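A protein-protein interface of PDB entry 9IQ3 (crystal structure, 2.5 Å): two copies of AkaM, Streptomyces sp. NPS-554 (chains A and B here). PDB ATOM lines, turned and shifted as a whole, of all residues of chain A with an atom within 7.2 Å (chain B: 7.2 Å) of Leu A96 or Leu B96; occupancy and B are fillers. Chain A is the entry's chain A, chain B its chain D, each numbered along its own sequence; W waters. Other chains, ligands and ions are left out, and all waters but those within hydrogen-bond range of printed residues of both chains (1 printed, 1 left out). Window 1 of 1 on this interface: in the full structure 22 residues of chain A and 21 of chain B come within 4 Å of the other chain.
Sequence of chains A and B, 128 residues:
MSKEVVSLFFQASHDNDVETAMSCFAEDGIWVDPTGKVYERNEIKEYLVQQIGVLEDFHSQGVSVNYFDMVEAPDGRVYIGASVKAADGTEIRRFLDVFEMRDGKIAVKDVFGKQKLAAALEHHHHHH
Val A32 touches Lys B114. Pro A34 touches Gly B113 (O to O, 3.7 Å). Leu B96 touches Tyr A79. Leu A96 touches Tyr B79 (CD1 to CE2, 3.6 Å). CD1 of Leu A96 touches CG2 of Val B98, 3.4 Å away. CE2 of Phe B112 touches CB of Leu A96, at 3.996 Å. Asp A110 touches Lys B114 (OD1 to CD, 3.8 Å). Phe B112 touches Phe A112. Pro B34 touches Gly A113. CG1 of Val B32 touches CE of Lys A114, 3.7 Å away.
Arg A94 touches Asp B110, and with the chains exchanged Asp A110 touches Arg B94. Leu A96 touches its own counterpart, Leu B96. Leu A96 touches Val B98, and with the chains exchanged Val A98 touches Leu B96. Leu A96 touches Phe B112, but with the chains exchanged Phe A112 does not touch Leu B96 (4.1 Å). Positions printed for both chains: 32, 34, 68, 79, 80, 81, 82, 94, 95, 96, 97, 98, 99, 110, 111, 112, 113 and 114. Of the 19 pairs that touch across the chains among the printed residues, 17 have their exchanged pair printed and touching as well.
O of Val B32 lies within hydrogen-bond range of N of Val B111 (2.9 Å). The backbone carbonyl oxygen (O) of Asp B110 lies within hydrogen-bond range of the backbone NH (N) of Val B98, at 3.1 Å. The backbone NH (N) of Phe B112 lies within hydrogen-bond range of the backbone carbonyl oxygen (O) of Leu B96 (2.8 Å). The backbone carbonyl oxygen (O) of Arg B94 is in hydrogen-bond range of the backbone NH (N) of Lys B114, 2.9 Å away. The backbone carbonyl oxygen (O) of Arg A94 lies within hydrogen-bond range of the backbone NH (N) of Lys A114, at 2.9 Å. O of Val A32 lies within hydrogen-bond range of N of Val A111 (2.9 Å).
Of the 18 printed residues of chain A, 10 touch a printed residue of chain B. Of the 18 printed residues of chain B, 10 touch a printed residue of chain A. Hydrophobic or aromatic side chains of chain B that line the printed part of chain A: Val B32, Tyr B79, Leu B96, Val B98 and Phe B112. Among the printed residues, Asp or Glu carboxylates within 4 Å of a Lys or Arg side-chain nitrogen of the other chain: Arg A94 with Asp B110 (2.7 Å) and Asp A110 with Arg B94 (2.7 Å).
Of the printed residues of chain B, Leu A96 touches Tyr B79, Leu B96, Val B98 and Phe B112. Leu B96 touches just these residues of chain A: Tyr A79, Leu A96 and Val A98. Printed residues of chain B within 4 Å of Tyr A79: Tyr B79 (3.96 Å) and Leu B96 (3.5 Å). Printed residues of chain A within 4 Å of Pro B34: Gly A113. Phe B95 touches none of the printed residues of chain A. Phe A99 touches none of the printed residues of chain B. The nearest residue of chain A that does not touch Leu B96 is Phe A112 (4.1 Å). The nearest printed residue of chain A that does not touch Val B98 is Phe A68 (5.5 Å).
Water W1 lies within hydrogen-bond range of the backbone carbonyl oxygen of Gly A113, the backbone NH of Gly B113 and the backbone carbonyl oxygen of Pro B34.
The side-chain carboxylate (OD2) of Asp A110 is in salt-bridge range of the guanidinium group (NH1) of Arg B94 (2.7 Å). NH1 of Arg A94 is in salt-bridge range of OD2 of Asp B110.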
ATOM      1  N   VAL A  32      14.542 -23.131 -13.771  1.00  0.00           N
ATOM      2  CA  VAL A  32      13.324 -23.808 -13.355  1.00  0.00           C
ATOM      3  C   VAL A  32      12.730 -24.459 -14.598  1.00  0.00           C
ATOM      4  O   VAL A  32      12.590 -23.793 -15.623  1.00  0.00           O
ATOM      5  CB  VAL A  32      12.318 -22.826 -12.719  1.00  0.00           C
ATOM      6  CG1 VAL A  32      11.304 -23.554 -11.857  1.00  0.00           C
ATOM      7  CG2 VAL A  32      13.008 -21.742 -11.901  1.00  0.00           C
ATOM      8  N   PRO A  34       9.783 -26.940 -16.834  1.00  0.00           N
ATOM      9  CA  PRO A  34       8.324 -26.893 -16.964  1.00  0.00           C
ATOM     10  C   PRO A  34       7.613 -27.291 -15.674  1.00  0.00           C
ATOM     11  O   PRO A  34       6.580 -26.724 -15.338  1.00  0.00           O
ATOM     12  CB  PRO A  34       8.032 -27.965 -18.024  1.00  0.00           C
ATOM     13  CG  PRO A  34       9.279 -28.000 -18.892  1.00  0.00           C
ATOM     14  CD  PRO A  34      10.425 -27.558 -18.006  1.00  0.00           C
ATOM     15  N   PHE A  68      11.132 -19.116 -32.432  1.00  0.00           N
ATOM     16  CA  PHE A  68      10.458 -17.948 -32.973  1.00  0.00           C
ATOM     17  C   PHE A  68      10.494 -16.787 -31.984  1.00  0.00           C
ATOM     18  O   PHE A  68      10.162 -16.950 -30.809  1.00  0.00           O
ATOM     19  CB  PHE A  68       9.040 -18.281 -33.456  1.00  0.00           C
ATOM     20  CG  PHE A  68       8.215 -19.173 -32.560  1.00  0.00           C
ATOM     21  CD1 PHE A  68       7.716 -18.714 -31.348  1.00  0.00           C
ATOM     22  CD2 PHE A  68       7.906 -20.469 -32.948  1.00  0.00           C
ATOM     23  CE1 PHE A  68       6.948 -19.537 -30.536  1.00  0.00           C
ATOM     24  CE2 PHE A  68       7.138 -21.293 -32.137  1.00  0.00           C
ATOM     25  CZ  PHE A  68       6.659 -20.824 -30.933  1.00  0.00           C
ATOM     26  N   TYR A  79      11.517 -12.907 -23.863  1.00  0.00           N
ATOM     27  CA  TYR A  79      10.693 -14.058 -24.186  1.00  0.00           C
ATOM     28  C   TYR A  79      11.154 -14.668 -25.505  1.00  0.00           C
ATOM     29  O   TYR A  79      11.555 -13.957 -26.425  1.00  0.00           O
ATOM     30  CB  TYR A  79       9.215 -13.668 -24.273  1.00  0.00           C
ATOM     31  CG  TYR A  79       8.659 -12.976 -23.053  1.00  0.00           C
ATOM     32  CD1 TYR A  79       8.882 -11.627 -22.824  1.00  0.00           C
ATOM     33  CD2 TYR A  79       7.882 -13.667 -22.139  1.00  0.00           C
ATOM     34  CE1 TYR A  79       8.370 -10.989 -21.706  1.00  0.00           C
ATOM     35  CE2 TYR A  79       7.359 -13.046 -21.017  1.00  0.00           C
ATOM     36  CZ  TYR A  79       7.603 -11.702 -20.800  1.00  0.00           C
ATOM     37  OH  TYR A  79       7.090 -11.080 -19.688  1.00  0.00           O
ATOM     38  N   ILE A  80      11.099 -16.001 -25.559  1.00  0.00           N
ATOM     39  CA  ILE A  80      11.285 -16.765 -26.780  1.00  0.00           C
ATOM     40  C   ILE A  80      10.404 -18.007 -26.673  1.00  0.00           C
ATOM     41  O   ILE A  80      10.082 -18.447 -25.568  1.00  0.00           O
ATOM     42  CB  ILE A  80      12.774 -17.104 -27.013  1.00  0.00           C
ATOM     43  CG1 ILE A  80      13.004 -17.809 -28.356  1.00  0.00           C
ATOM     44  CG2 ILE A  80      13.358 -17.887 -25.843  1.00  0.00           C
ATOM     45  CD1 ILE A  80      14.463 -18.056 -28.688  1.00  0.00           C
ATOM     46  N   GLY A  81       9.993 -18.539 -27.829  1.00  0.00           N
ATOM     47  CA  GLY A  81       9.181 -19.741 -27.873  1.00  0.00           C
ATOM     48  C   GLY A  81       9.807 -20.809 -28.763  1.00  0.00           C
ATOM     49  O   GLY A  81      10.543 -20.491 -29.697  1.00  0.00           O
ATOM     50  N   ALA A  82       9.493 -22.072 -28.452  1.00  0.00           N
ATOM     51  CA  ALA A  82       9.991 -23.217 -29.193  1.00  0.00           C
ATOM     52  C   ALA A  82       8.822 -24.111 -29.603  1.00  0.00           C
ATOM     53  O   ALA A  82       7.837 -24.227 -28.876  1.00  0.00           O
ATOM     54  CB  ALA A  82      10.994 -23.972 -28.355  1.00  0.00           C
ATOM     55  N   ARG A  94       5.378 -27.965 -27.376  1.00  0.00           N
ATOM     56  CA  ARG A  94       5.761 -26.561 -27.382  1.00  0.00           C
ATOM     57  C   ARG A  94       6.453 -26.237 -26.061  1.00  0.00           C
ATOM     58  O   ARG A  94       6.199 -26.881 -25.046  1.00  0.00           O
ATOM     59  CB  ARG A  94       4.543 -25.640 -27.521  1.00  0.00           C
ATOM     60  CG  ARG A  94       3.900 -25.623 -28.900  1.00  0.00           C
ATOM     61  CD  ARG A  94       2.957 -24.440 -29.034  1.00  0.00           C
ATOM     62  NE  ARG A  94       2.309 -24.360 -30.337  1.00  0.00           N
ATOM     63  CZ  ARG A  94       1.029 -24.060 -30.538  1.00  0.00           C
ATOM     64  NH1 ARG A  94       0.248 -23.753 -29.518  1.00  0.00           N
ATOM     65  NH2 ARG A  94       0.539 -24.049 -31.766  1.00  0.00           N
ATOM     66  N   PHE A  95       7.324 -25.223 -26.088  1.00  0.00           N
ATOM     67  CA  PHE A  95       8.023 -24.762 -24.900  1.00  0.00           C
ATOM     68  C   PHE A  95       8.138 -23.243 -24.963  1.00  0.00           C
ATOM     69  O   PHE A  95       8.193 -22.668 -26.052  1.00  0.00           O
ATOM     70  CB  PHE A  95       9.430 -25.366 -24.826  1.00  0.00           C
ATOM     71  CG  PHE A  95       9.496 -26.871 -24.746  1.00  0.00           C
ATOM     72  CD1 PHE A  95       9.120 -27.548 -23.593  1.00  0.00           C
ATOM     73  CD2 PHE A  95       9.941 -27.617 -25.829  1.00  0.00           C
ATOM     74  CE1 PHE A  95       9.183 -28.933 -23.526  1.00  0.00           C
ATOM     75  CE2 PHE A  95      10.009 -29.002 -25.759  1.00  0.00           C
ATOM     76  CZ  PHE A  95       9.625 -29.658 -24.610  1.00  0.00           C
ATOM     77  N   LEU A  96       8.183 -22.605 -23.788  1.00  0.00           N
ATOM     78  CA  LEU A  96       8.457 -21.180 -23.725  1.00  0.00           C
ATOM     79  C   LEU A  96       9.404 -20.866 -22.569  1.00  0.00           C
ATOM     80  O   LEU A  96       9.355 -21.518 -21.530  1.00  0.00           O
ATOM     81  CB  LEU A  96       7.153 -20.405 -23.542  1.00  0.00           C
ATOM     82  CG  LEU A  96       7.378 -18.905 -23.379  1.00  0.00           C
ATOM     83  CD1 LEU A  96       6.610 -18.102 -24.417  1.00  0.00           C
ATOM     84  CD2 LEU A  96       7.075 -18.460 -21.962  1.00  0.00           C
ATOM     85  N   ASP A  97      10.208 -19.810 -22.756  1.00  0.00           N
ATOM     86  CA  ASP A  97      11.174 -19.342 -21.777  1.00  0.00           C
ATOM     87  C   ASP A  97      10.930 -17.865 -21.462  1.00  0.00           C
ATOM     88  O   ASP A  97      10.682 -17.063 -22.363  1.00  0.00           O
ATOM     89  CB  ASP A  97      12.599 -19.548 -22.295  1.00  0.00           C
ATOM     90  CG  ASP A  97      12.940 -21.007 -22.555  1.00  0.00           C
ATOM     91  OD1 ASP A  97      12.200 -21.888 -22.054  1.00  0.00           O
ATOM     92  OD2 ASP A  97      13.930 -21.254 -23.273  1.00  0.00           O
ATOM     93  N   VAL A  98      10.997 -17.534 -20.164  1.00  0.00           N
ATOM     94  CA  VAL A  98      11.063 -16.162 -19.678  1.00  0.00           C
ATOM     95  C   VAL A  98      12.368 -16.014 -18.898  1.00  0.00           C
ATOM     96  O   VAL A  98      12.663 -16.826 -18.022  1.00  0.00           O
ATOM     97  CB  VAL A  98       9.852 -15.780 -18.802  1.00  0.00           C
ATOM     98  CG1 VAL A  98       9.859 -14.298 -18.440  1.00  0.00           C
ATOM     99  CG2 VAL A  98       8.533 -16.152 -19.456  1.00  0.00           C
ATOM    100  N   PHE A  99      13.138 -14.970 -19.237  1.00  0.00           N
ATOM    101  CA  PHE A  99      14.434 -14.724 -18.629  1.00  0.00           C
ATOM    102  C   PHE A  99      14.367 -13.469 -17.765  1.00  0.00           C
ATOM    103  O   PHE A  99      14.304 -12.358 -18.288  1.00  0.00           O
ATOM    104  CB  PHE A  99      15.502 -14.520 -19.707  1.00  0.00           C
ATOM    105  CG  PHE A  99      15.936 -15.749 -20.469  1.00  0.00           C
ATOM    106  CD1 PHE A  99      15.136 -16.300 -21.458  1.00  0.00           C
ATOM    107  CD2 PHE A  99      17.176 -16.327 -20.227  1.00  0.00           C
ATOM    108  CE1 PHE A  99      15.554 -17.417 -22.170  1.00  0.00           C
ATOM    109  CE2 PHE A  99      17.590 -17.446 -20.935  1.00  0.00           C
ATOM    110  CZ  PHE A  99      16.779 -17.990 -21.906  1.00  0.00           C
ATOM    111  N   ASP A 110      13.289 -19.716 -16.918  1.00  0.00           N
ATOM    112  CA  ASP A 110      12.000 -20.247 -16.507  1.00  0.00           C
ATOM    113  C   ASP A 110      11.311 -20.879 -17.711  1.00  0.00           C
ATOM    114  O   ASP A 110      10.789 -20.174 -18.576  1.00  0.00           O
ATOM    115  CB  ASP A 110      11.144 -19.156 -15.856  1.00  0.00           C
ATOM    116  CG  ASP A 110      10.045 -19.681 -14.948  1.00  0.00           C
ATOM    117  OD1 ASP A 110      10.015 -20.908 -14.700  1.00  0.00           O
ATOM    118  OD2 ASP A 110       9.227 -18.854 -14.487  1.00  0.00           O
ATOM    119  N   VAL A 111      11.326 -22.218 -17.754  1.00  0.00           N
ATOM    120  CA  VAL A 111      10.766 -22.948 -18.879  1.00  0.00           C
ATOM    121  C   VAL A 111       9.356 -23.407 -18.517  1.00  0.00           C
ATOM    122  O   VAL A 111       9.131 -23.938 -17.432  1.00  0.00           O
ATOM    123  CB  VAL A 111      11.663 -24.124 -19.316  1.00  0.00           C
ATOM    124  CG1 VAL A 111      11.184 -24.749 -20.618  1.00  0.00           C
ATOM    125  CG2 VAL A 111      13.124 -23.712 -19.447  1.00  0.00           C
ATOM    126  N   PHE A 112       8.418 -23.153 -19.436  1.00  0.00           N
ATOM    127  CA  PHE A 112       7.044 -23.620 -19.355  1.00  0.00           C
ATOM    128  C   PHE A 112       6.807 -24.610 -20.495  1.00  0.00           C
ATOM    129  O   PHE A 112       7.259 -24.378 -21.615  1.00  0.00           O
ATOM    130  CB  PHE A 112       6.085 -22.431 -19.464  1.00  0.00           C
ATOM    131  CG  PHE A 112       6.176 -21.398 -18.365  1.00  0.00           C
ATOM    132  CD1 PHE A 112       5.654 -21.651 -17.102  1.00  0.00           C
ATOM    133  CD2 PHE A 112       6.757 -20.159 -18.596  1.00  0.00           C
ATOM    134  CE1 PHE A 112       5.722 -20.695 -16.100  1.00  0.00           C
ATOM    135  CE2 PHE A 112       6.830 -19.205 -17.592  1.00  0.00           C
ATOM    136  CZ  PHE A 112       6.316 -19.477 -16.343  1.00  0.00           C
ATOM    137  N   GLY A 113       6.099 -25.710 -20.202  1.00  0.00           N
ATOM    138  CA  GLY A 113       5.919 -26.786 -21.163  1.00  0.00           C
ATOM    139  C   GLY A 113       4.469 -26.947 -21.620  1.00  0.00           C
ATOM    140  O   GLY A 113       3.539 -26.805 -20.824  1.00  0.00           O
ATOM    141  N   LYS A 114       4.292 -27.234 -22.917  1.00  0.00           N
ATOM    142  CA  LYS A 114       3.001 -27.625 -23.461  1.00  0.00           C
ATOM    143  C   LYS A 114       2.977 -29.143 -23.606  1.00  0.00           C
ATOM    144  O   LYS A 114       3.177 -29.689 -24.696  1.00  0.00           O
ATOM    145  CB  LYS A 114       2.679 -26.918 -24.783  1.00  0.00           C
ATOM    146  CG  LYS A 114       1.261 -27.136 -25.298  1.00  0.00           C
ATOM    147  CD  LYS A 114       1.047 -26.671 -26.722  1.00  0.00           C
ATOM    148  CE  LYS A 114      -0.294 -27.081 -27.290  1.00  0.00           C
ATOM    149  NZ  LYS A 114      -0.497 -26.544 -28.657  1.00  0.00           N
ATOM    150  N   VAL B  32      -5.850 -23.114 -25.567  1.00  0.00           N
ATOM    151  CA  VAL B  32      -5.137 -24.295 -25.108  1.00  0.00           C
ATOM    152  C   VAL B  32      -4.638 -23.994 -23.700  1.00  0.00           C
ATOM    153  O   VAL B  32      -4.034 -22.947 -23.486  1.00  0.00           O
ATOM    154  CB  VAL B  32      -3.959 -24.648 -26.040  1.00  0.00           C
ATOM    155  CG1 VAL B  32      -3.529 -26.099 -25.866  1.00  0.00           C
ATOM    156  CG2 VAL B  32      -4.272 -24.361 -27.503  1.00  0.00           C
ATOM    157  N   PRO B  34      -2.643 -24.932 -19.831  1.00  0.00           N
ATOM    158  CA  PRO B  34      -1.309 -25.425 -19.483  1.00  0.00           C
ATOM    159  C   PRO B  34      -1.104 -26.881 -19.887  1.00  0.00           C
ATOM    160  O   PRO B  34      -0.014 -27.254 -20.309  1.00  0.00           O
ATOM    161  CB  PRO B  34      -1.292 -25.347 -17.950  1.00  0.00           C
ATOM    162  CG  PRO B  34      -2.239 -24.209 -17.611  1.00  0.00           C
ATOM    163  CD  PRO B  34      -3.244 -24.137 -18.745  1.00  0.00           C
ATOM    164  N   PHE B  68       2.477  -8.756 -15.547  1.00  0.00           N
ATOM    165  CA  PHE B  68       3.668  -8.006 -15.914  1.00  0.00           C
ATOM    166  C   PHE B  68       3.929  -8.081 -17.416  1.00  0.00           C
ATOM    167  O   PHE B  68       3.930  -9.161 -18.004  1.00  0.00           O
ATOM    168  CB  PHE B  68       4.882  -8.424 -15.072  1.00  0.00           C
ATOM    169  CG  PHE B  68       5.072  -9.906 -14.853  1.00  0.00           C
ATOM    170  CD1 PHE B  68       5.472 -10.744 -15.885  1.00  0.00           C
ATOM    171  CD2 PHE B  68       4.885 -10.461 -13.595  1.00  0.00           C
ATOM    172  CE1 PHE B  68       5.655 -12.102 -15.670  1.00  0.00           C
ATOM    173  CE2 PHE B  68       5.069 -11.819 -13.380  1.00  0.00           C
ATOM    174  CZ  PHE B  68       5.452 -12.638 -14.418  1.00  0.00           C
ATOM    175  N   TYR B  79       3.068 -11.469 -25.781  1.00  0.00           N
ATOM    176  CA  TYR B  79       3.382 -12.199 -24.567  1.00  0.00           C
ATOM    177  C   TYR B  79       2.977 -11.378 -23.349  1.00  0.00           C
ATOM    178  O   TYR B  79       3.094 -10.153 -23.344  1.00  0.00           O
ATOM    179  CB  TYR B  79       4.874 -12.537 -24.503  1.00  0.00           C
ATOM    180  CG  TYR B  79       5.411 -13.294 -25.691  1.00  0.00           C
ATOM    181  CD1 TYR B  79       5.731 -12.640 -26.873  1.00  0.00           C
ATOM    182  CD2 TYR B  79       5.627 -14.662 -25.627  1.00  0.00           C
ATOM    183  CE1 TYR B  79       6.231 -13.329 -27.967  1.00  0.00           C
ATOM    184  CE2 TYR B  79       6.126 -15.365 -26.712  1.00  0.00           C
ATOM    185  CZ  TYR B  79       6.431 -14.696 -27.885  1.00  0.00           C
ATOM    186  OH  TYR B  79       6.926 -15.390 -28.960  1.00  0.00           O
ATOM    187  N   ILE B  80       2.484 -12.087 -22.331  1.00  0.00           N
ATOM    188  CA  ILE B  80       2.235 -11.535 -21.011  1.00  0.00           C
ATOM    189  C   ILE B  80       2.480 -12.654 -20.004  1.00  0.00           C
ATOM    190  O   ILE B  80       2.366 -13.833 -20.344  1.00  0.00           O
ATOM    191  CB  ILE B  80       0.816 -10.932 -20.908  1.00  0.00           C
ATOM    192  CG1 ILE B  80       0.585 -10.237 -19.560  1.00  0.00           C
ATOM    193  CG2 ILE B  80      -0.256 -11.971 -21.219  1.00  0.00           C
ATOM    194  CD1 ILE B  80      -0.760  -9.562 -19.409  1.00  0.00           C
ATOM    195  N   GLY B  81       2.846 -12.270 -18.778  1.00  0.00           N
ATOM    196  CA  GLY B  81       3.071 -13.227 -17.712  1.00  0.00           C
ATOM    197  C   GLY B  81       2.240 -12.897 -16.476  1.00  0.00           C
ATOM    198  O   GLY B  81       1.899 -11.738 -16.237  1.00  0.00           O
ATOM    199  N   ALA B  82       1.930 -13.941 -15.699  1.00  0.00           N
ATOM    200  CA  ALA B  82       1.155 -13.820 -14.477  1.00  0.00           C
ATOM    201  C   ALA B  82       1.901 -14.499 -13.332  1.00  0.00           C
ATOM    202  O   ALA B  82       2.584 -15.500 -13.537  1.00  0.00           O
ATOM    203  CB  ALA B  82      -0.214 -14.423 -14.677  1.00  0.00           C
ATOM    204  N   ARG B  94       2.957 -19.650 -11.336  1.00  0.00           N
ATOM    205  CA  ARG B  94       3.186 -18.720 -12.431  1.00  0.00           C
ATOM    206  C   ARG B  94       2.435 -19.220 -13.661  1.00  0.00           C
ATOM    207  O   ARG B  94       2.193 -20.416 -13.807  1.00  0.00           O
ATOM    208  CB  ARG B  94       4.674 -18.610 -12.778  1.00  0.00           C
ATOM    209  CG  ARG B  94       5.523 -17.867 -11.757  1.00  0.00           C
ATOM    210  CD  ARG B  94       6.857 -17.453 -12.356  1.00  0.00           C
ATOM    211  NE  ARG B  94       7.716 -16.736 -11.422  1.00  0.00           N
ATOM    212  CZ  ARG B  94       9.022 -16.938 -11.274  1.00  0.00           C
ATOM    213  NH1 ARG B  94       9.658 -17.802 -12.044  1.00  0.00           N
ATOM    214  NH2 ARG B  94       9.698 -16.254 -10.366  1.00  0.00           N
ATOM    215  N   PHE B  95       2.078 -18.283 -14.544  1.00  0.00           N
ATOM    216  CA  PHE B  95       1.413 -18.603 -15.796  1.00  0.00           C
ATOM    217  C   PHE B  95       1.952 -17.682 -16.883  1.00  0.00           C
ATOM    218  O   PHE B  95       2.352 -16.553 -16.598  1.00  0.00           O
ATOM    219  CB  PHE B  95      -0.100 -18.404 -15.674  1.00  0.00           C
ATOM    220  CG  PHE B  95      -0.797 -19.260 -14.646  1.00  0.00           C
ATOM    221  CD1 PHE B  95      -0.973 -20.622 -14.846  1.00  0.00           C
ATOM    222  CD2 PHE B  95      -1.288 -18.703 -13.475  1.00  0.00           C
ATOM    223  CE1 PHE B  95      -1.615 -21.408 -13.900  1.00  0.00           C
ATOM    224  CE2 PHE B  95      -1.934 -19.487 -12.530  1.00  0.00           C
ATOM    225  CZ  PHE B  95      -2.097 -20.838 -12.742  1.00  0.00           C
ATOM    226  N   LEU B  96       1.959 -18.180 -18.123  1.00  0.00           N
ATOM    227  CA  LEU B  96       2.302 -17.341 -19.256  1.00  0.00           C
ATOM    228  C   LEU B  96       1.370 -17.620 -20.430  1.00  0.00           C
ATOM    229  O   LEU B  96       0.939 -18.755 -20.629  1.00  0.00           O
ATOM    230  CB  LEU B  96       3.749 -17.592 -19.676  1.00  0.00           C
ATOM    231  CG  LEU B  96       4.146 -16.807 -20.923  1.00  0.00           C
ATOM    232  CD1 LEU B  96       5.361 -15.931 -20.676  1.00  0.00           C
ATOM    233  CD2 LEU B  96       4.323 -17.728 -22.116  1.00  0.00           C
ATOM    234  N   ASP B  97       1.136 -16.572 -21.232  1.00  0.00           N
ATOM    235  CA  ASP B  97       0.283 -16.627 -22.406  1.00  0.00           C
ATOM    236  C   ASP B  97       1.052 -16.155 -23.637  1.00  0.00           C
ATOM    237  O   ASP B  97       1.785 -15.166 -23.580  1.00  0.00           O
ATOM    238  CB  ASP B  97      -0.969 -15.773 -22.199  1.00  0.00           C
ATOM    239  CG  ASP B  97      -1.828 -16.233 -21.035  1.00  0.00           C
ATOM    240  OD1 ASP B  97      -1.640 -17.383 -20.588  1.00  0.00           O
ATOM    241  OD2 ASP B  97      -2.663 -15.429 -20.571  1.00  0.00           O
ATOM    242  N   VAL B  98       0.873 -16.893 -24.742  1.00  0.00           N
ATOM    243  CA  VAL B  98       1.289 -16.474 -26.072  1.00  0.00           C
ATOM    244  C   VAL B  98       0.037 -16.414 -26.945  1.00  0.00           C
ATOM    245  O   VAL B  98      -0.737 -17.371 -26.988  1.00  0.00           O
ATOM    246  CB  VAL B  98       2.343 -17.420 -26.685  1.00  0.00           C
ATOM    247  CG1 VAL B  98       2.884 -16.882 -28.005  1.00  0.00           C
ATOM    248  CG2 VAL B  98       3.485 -17.706 -25.725  1.00  0.00           C
ATOM    249  N   PHE B  99      -0.142 -15.280 -27.631  1.00  0.00           N
ATOM    250  CA  PHE B  99      -1.310 -15.044 -28.464  1.00  0.00           C
ATOM    251  C   PHE B  99      -0.895 -15.019 -29.932  1.00  0.00           C
ATOM    252  O   PHE B  99      -0.271 -14.062 -30.383  1.00  0.00           O
ATOM    253  CB  PHE B  99      -1.961 -13.702 -28.115  1.00  0.00           C
ATOM    254  CG  PHE B  99      -2.707 -13.635 -26.806  1.00  0.00           C
ATOM    255  CD1 PHE B  99      -2.031 -13.548 -25.597  1.00  0.00           C
ATOM    256  CD2 PHE B  99      -4.094 -13.608 -26.787  1.00  0.00           C
ATOM    257  CE1 PHE B  99      -2.727 -13.464 -24.400  1.00  0.00           C
ATOM    258  CE2 PHE B  99      -4.790 -13.530 -25.589  1.00  0.00           C
ATOM    259  CZ  PHE B  99      -4.105 -13.458 -24.397  1.00  0.00           C
ATOM    260  N   ASP B 110      -2.698 -19.497 -25.738  1.00  0.00           N
ATOM    261  CA  ASP B 110      -1.856 -20.622 -25.370  1.00  0.00           C
ATOM    262  C   ASP B 110      -1.269 -20.377 -23.983  1.00  0.00           C
ATOM    263  O   ASP B 110      -0.339 -19.580 -23.827  1.00  0.00           O
ATOM    264  CB  ASP B 110      -0.771 -20.860 -26.423  1.00  0.00           C
ATOM    265  CG  ASP B 110      -0.185 -22.266 -26.414  1.00  0.00           C
ATOM    266  OD1 ASP B 110      -0.720 -23.127 -25.674  1.00  0.00           O
ATOM    267  OD2 ASP B 110       0.797 -22.492 -27.153  1.00  0.00           O
ATOM    268  N   VAL B 111      -1.835 -21.067 -22.983  1.00  0.00           N
ATOM    269  CA  VAL B 111      -1.427 -20.874 -21.602  1.00  0.00           C
ATOM    270  C   VAL B 111      -0.443 -21.976 -21.222  1.00  0.00           C
ATOM    271  O   VAL B 111      -0.681 -23.152 -21.497  1.00  0.00           O
ATOM    272  CB  VAL B 111      -2.630 -20.814 -20.640  1.00  0.00           C
ATOM    273  CG1 VAL B 111      -2.210 -20.400 -19.236  1.00  0.00           C
ATOM    274  CG2 VAL B 111      -3.726 -19.891 -21.152  1.00  0.00           C
ATOM    275  N   PHE B 112       0.678 -21.559 -20.619  1.00  0.00           N
ATOM    276  CA  PHE B 112       1.682 -22.445 -20.058  1.00  0.00           C
ATOM    277  C   PHE B 112       1.701 -22.247 -18.543  1.00  0.00           C
ATOM    278  O   PHE B 112       1.623 -21.115 -18.067  1.00  0.00           O
ATOM    279  CB  PHE B 112       3.052 -22.128 -20.662  1.00  0.00           C
ATOM    280  CG  PHE B 112       3.187 -22.337 -22.153  1.00  0.00           C
ATOM    281  CD1 PHE B 112       3.290 -23.613 -22.692  1.00  0.00           C
ATOM    282  CD2 PHE B 112       3.244 -21.253 -23.018  1.00  0.00           C
ATOM    283  CE1 PHE B 112       3.431 -23.798 -24.061  1.00  0.00           C
ATOM    284  CE2 PHE B 112       3.386 -21.436 -24.387  1.00  0.00           C
ATOM    285  CZ  PHE B 112       3.480 -22.711 -24.906  1.00  0.00           C
ATOM    286  N   GLY B 113       1.804 -23.357 -17.796  1.00  0.00           N
ATOM    287  CA  GLY B 113       1.697 -23.317 -16.345  1.00  0.00           C
ATOM    288  C   GLY B 113       2.996 -23.692 -15.638  1.00  0.00           C
ATOM    289  O   GLY B 113       3.697 -24.607 -16.072  1.00  0.00           O
ATOM    290  N   LYS B 114       3.313 -22.958 -14.562  1.00  0.00           N
ATOM    291  CA  LYS B 114       4.439 -23.287 -13.702  1.00  0.00           C
ATOM    292  C   LYS B 114       3.906 -23.991 -12.459  1.00  0.00           C
ATOM    293  O   LYS B 114       3.779 -23.394 -11.391  1.00  0.00           O
ATOM    294  CB  LYS B 114       5.284 -22.059 -13.343  1.00  0.00           C
ATOM    295  CG  LYS B 114       6.596 -22.374 -12.630  1.00  0.00           C
ATOM    296  CD  LYS B 114       7.286 -21.163 -12.042  1.00  0.00           C
ATOM    297  CE  LYS B 114       8.404 -21.522 -11.086  1.00  0.00           C
ATOM    298  NZ  LYS B 114       9.035 -20.318 -10.494  1.00  0.00           N
HETATM  299  O   HOH W   1       2.212 -26.032 -18.810  1.00  0.00           O
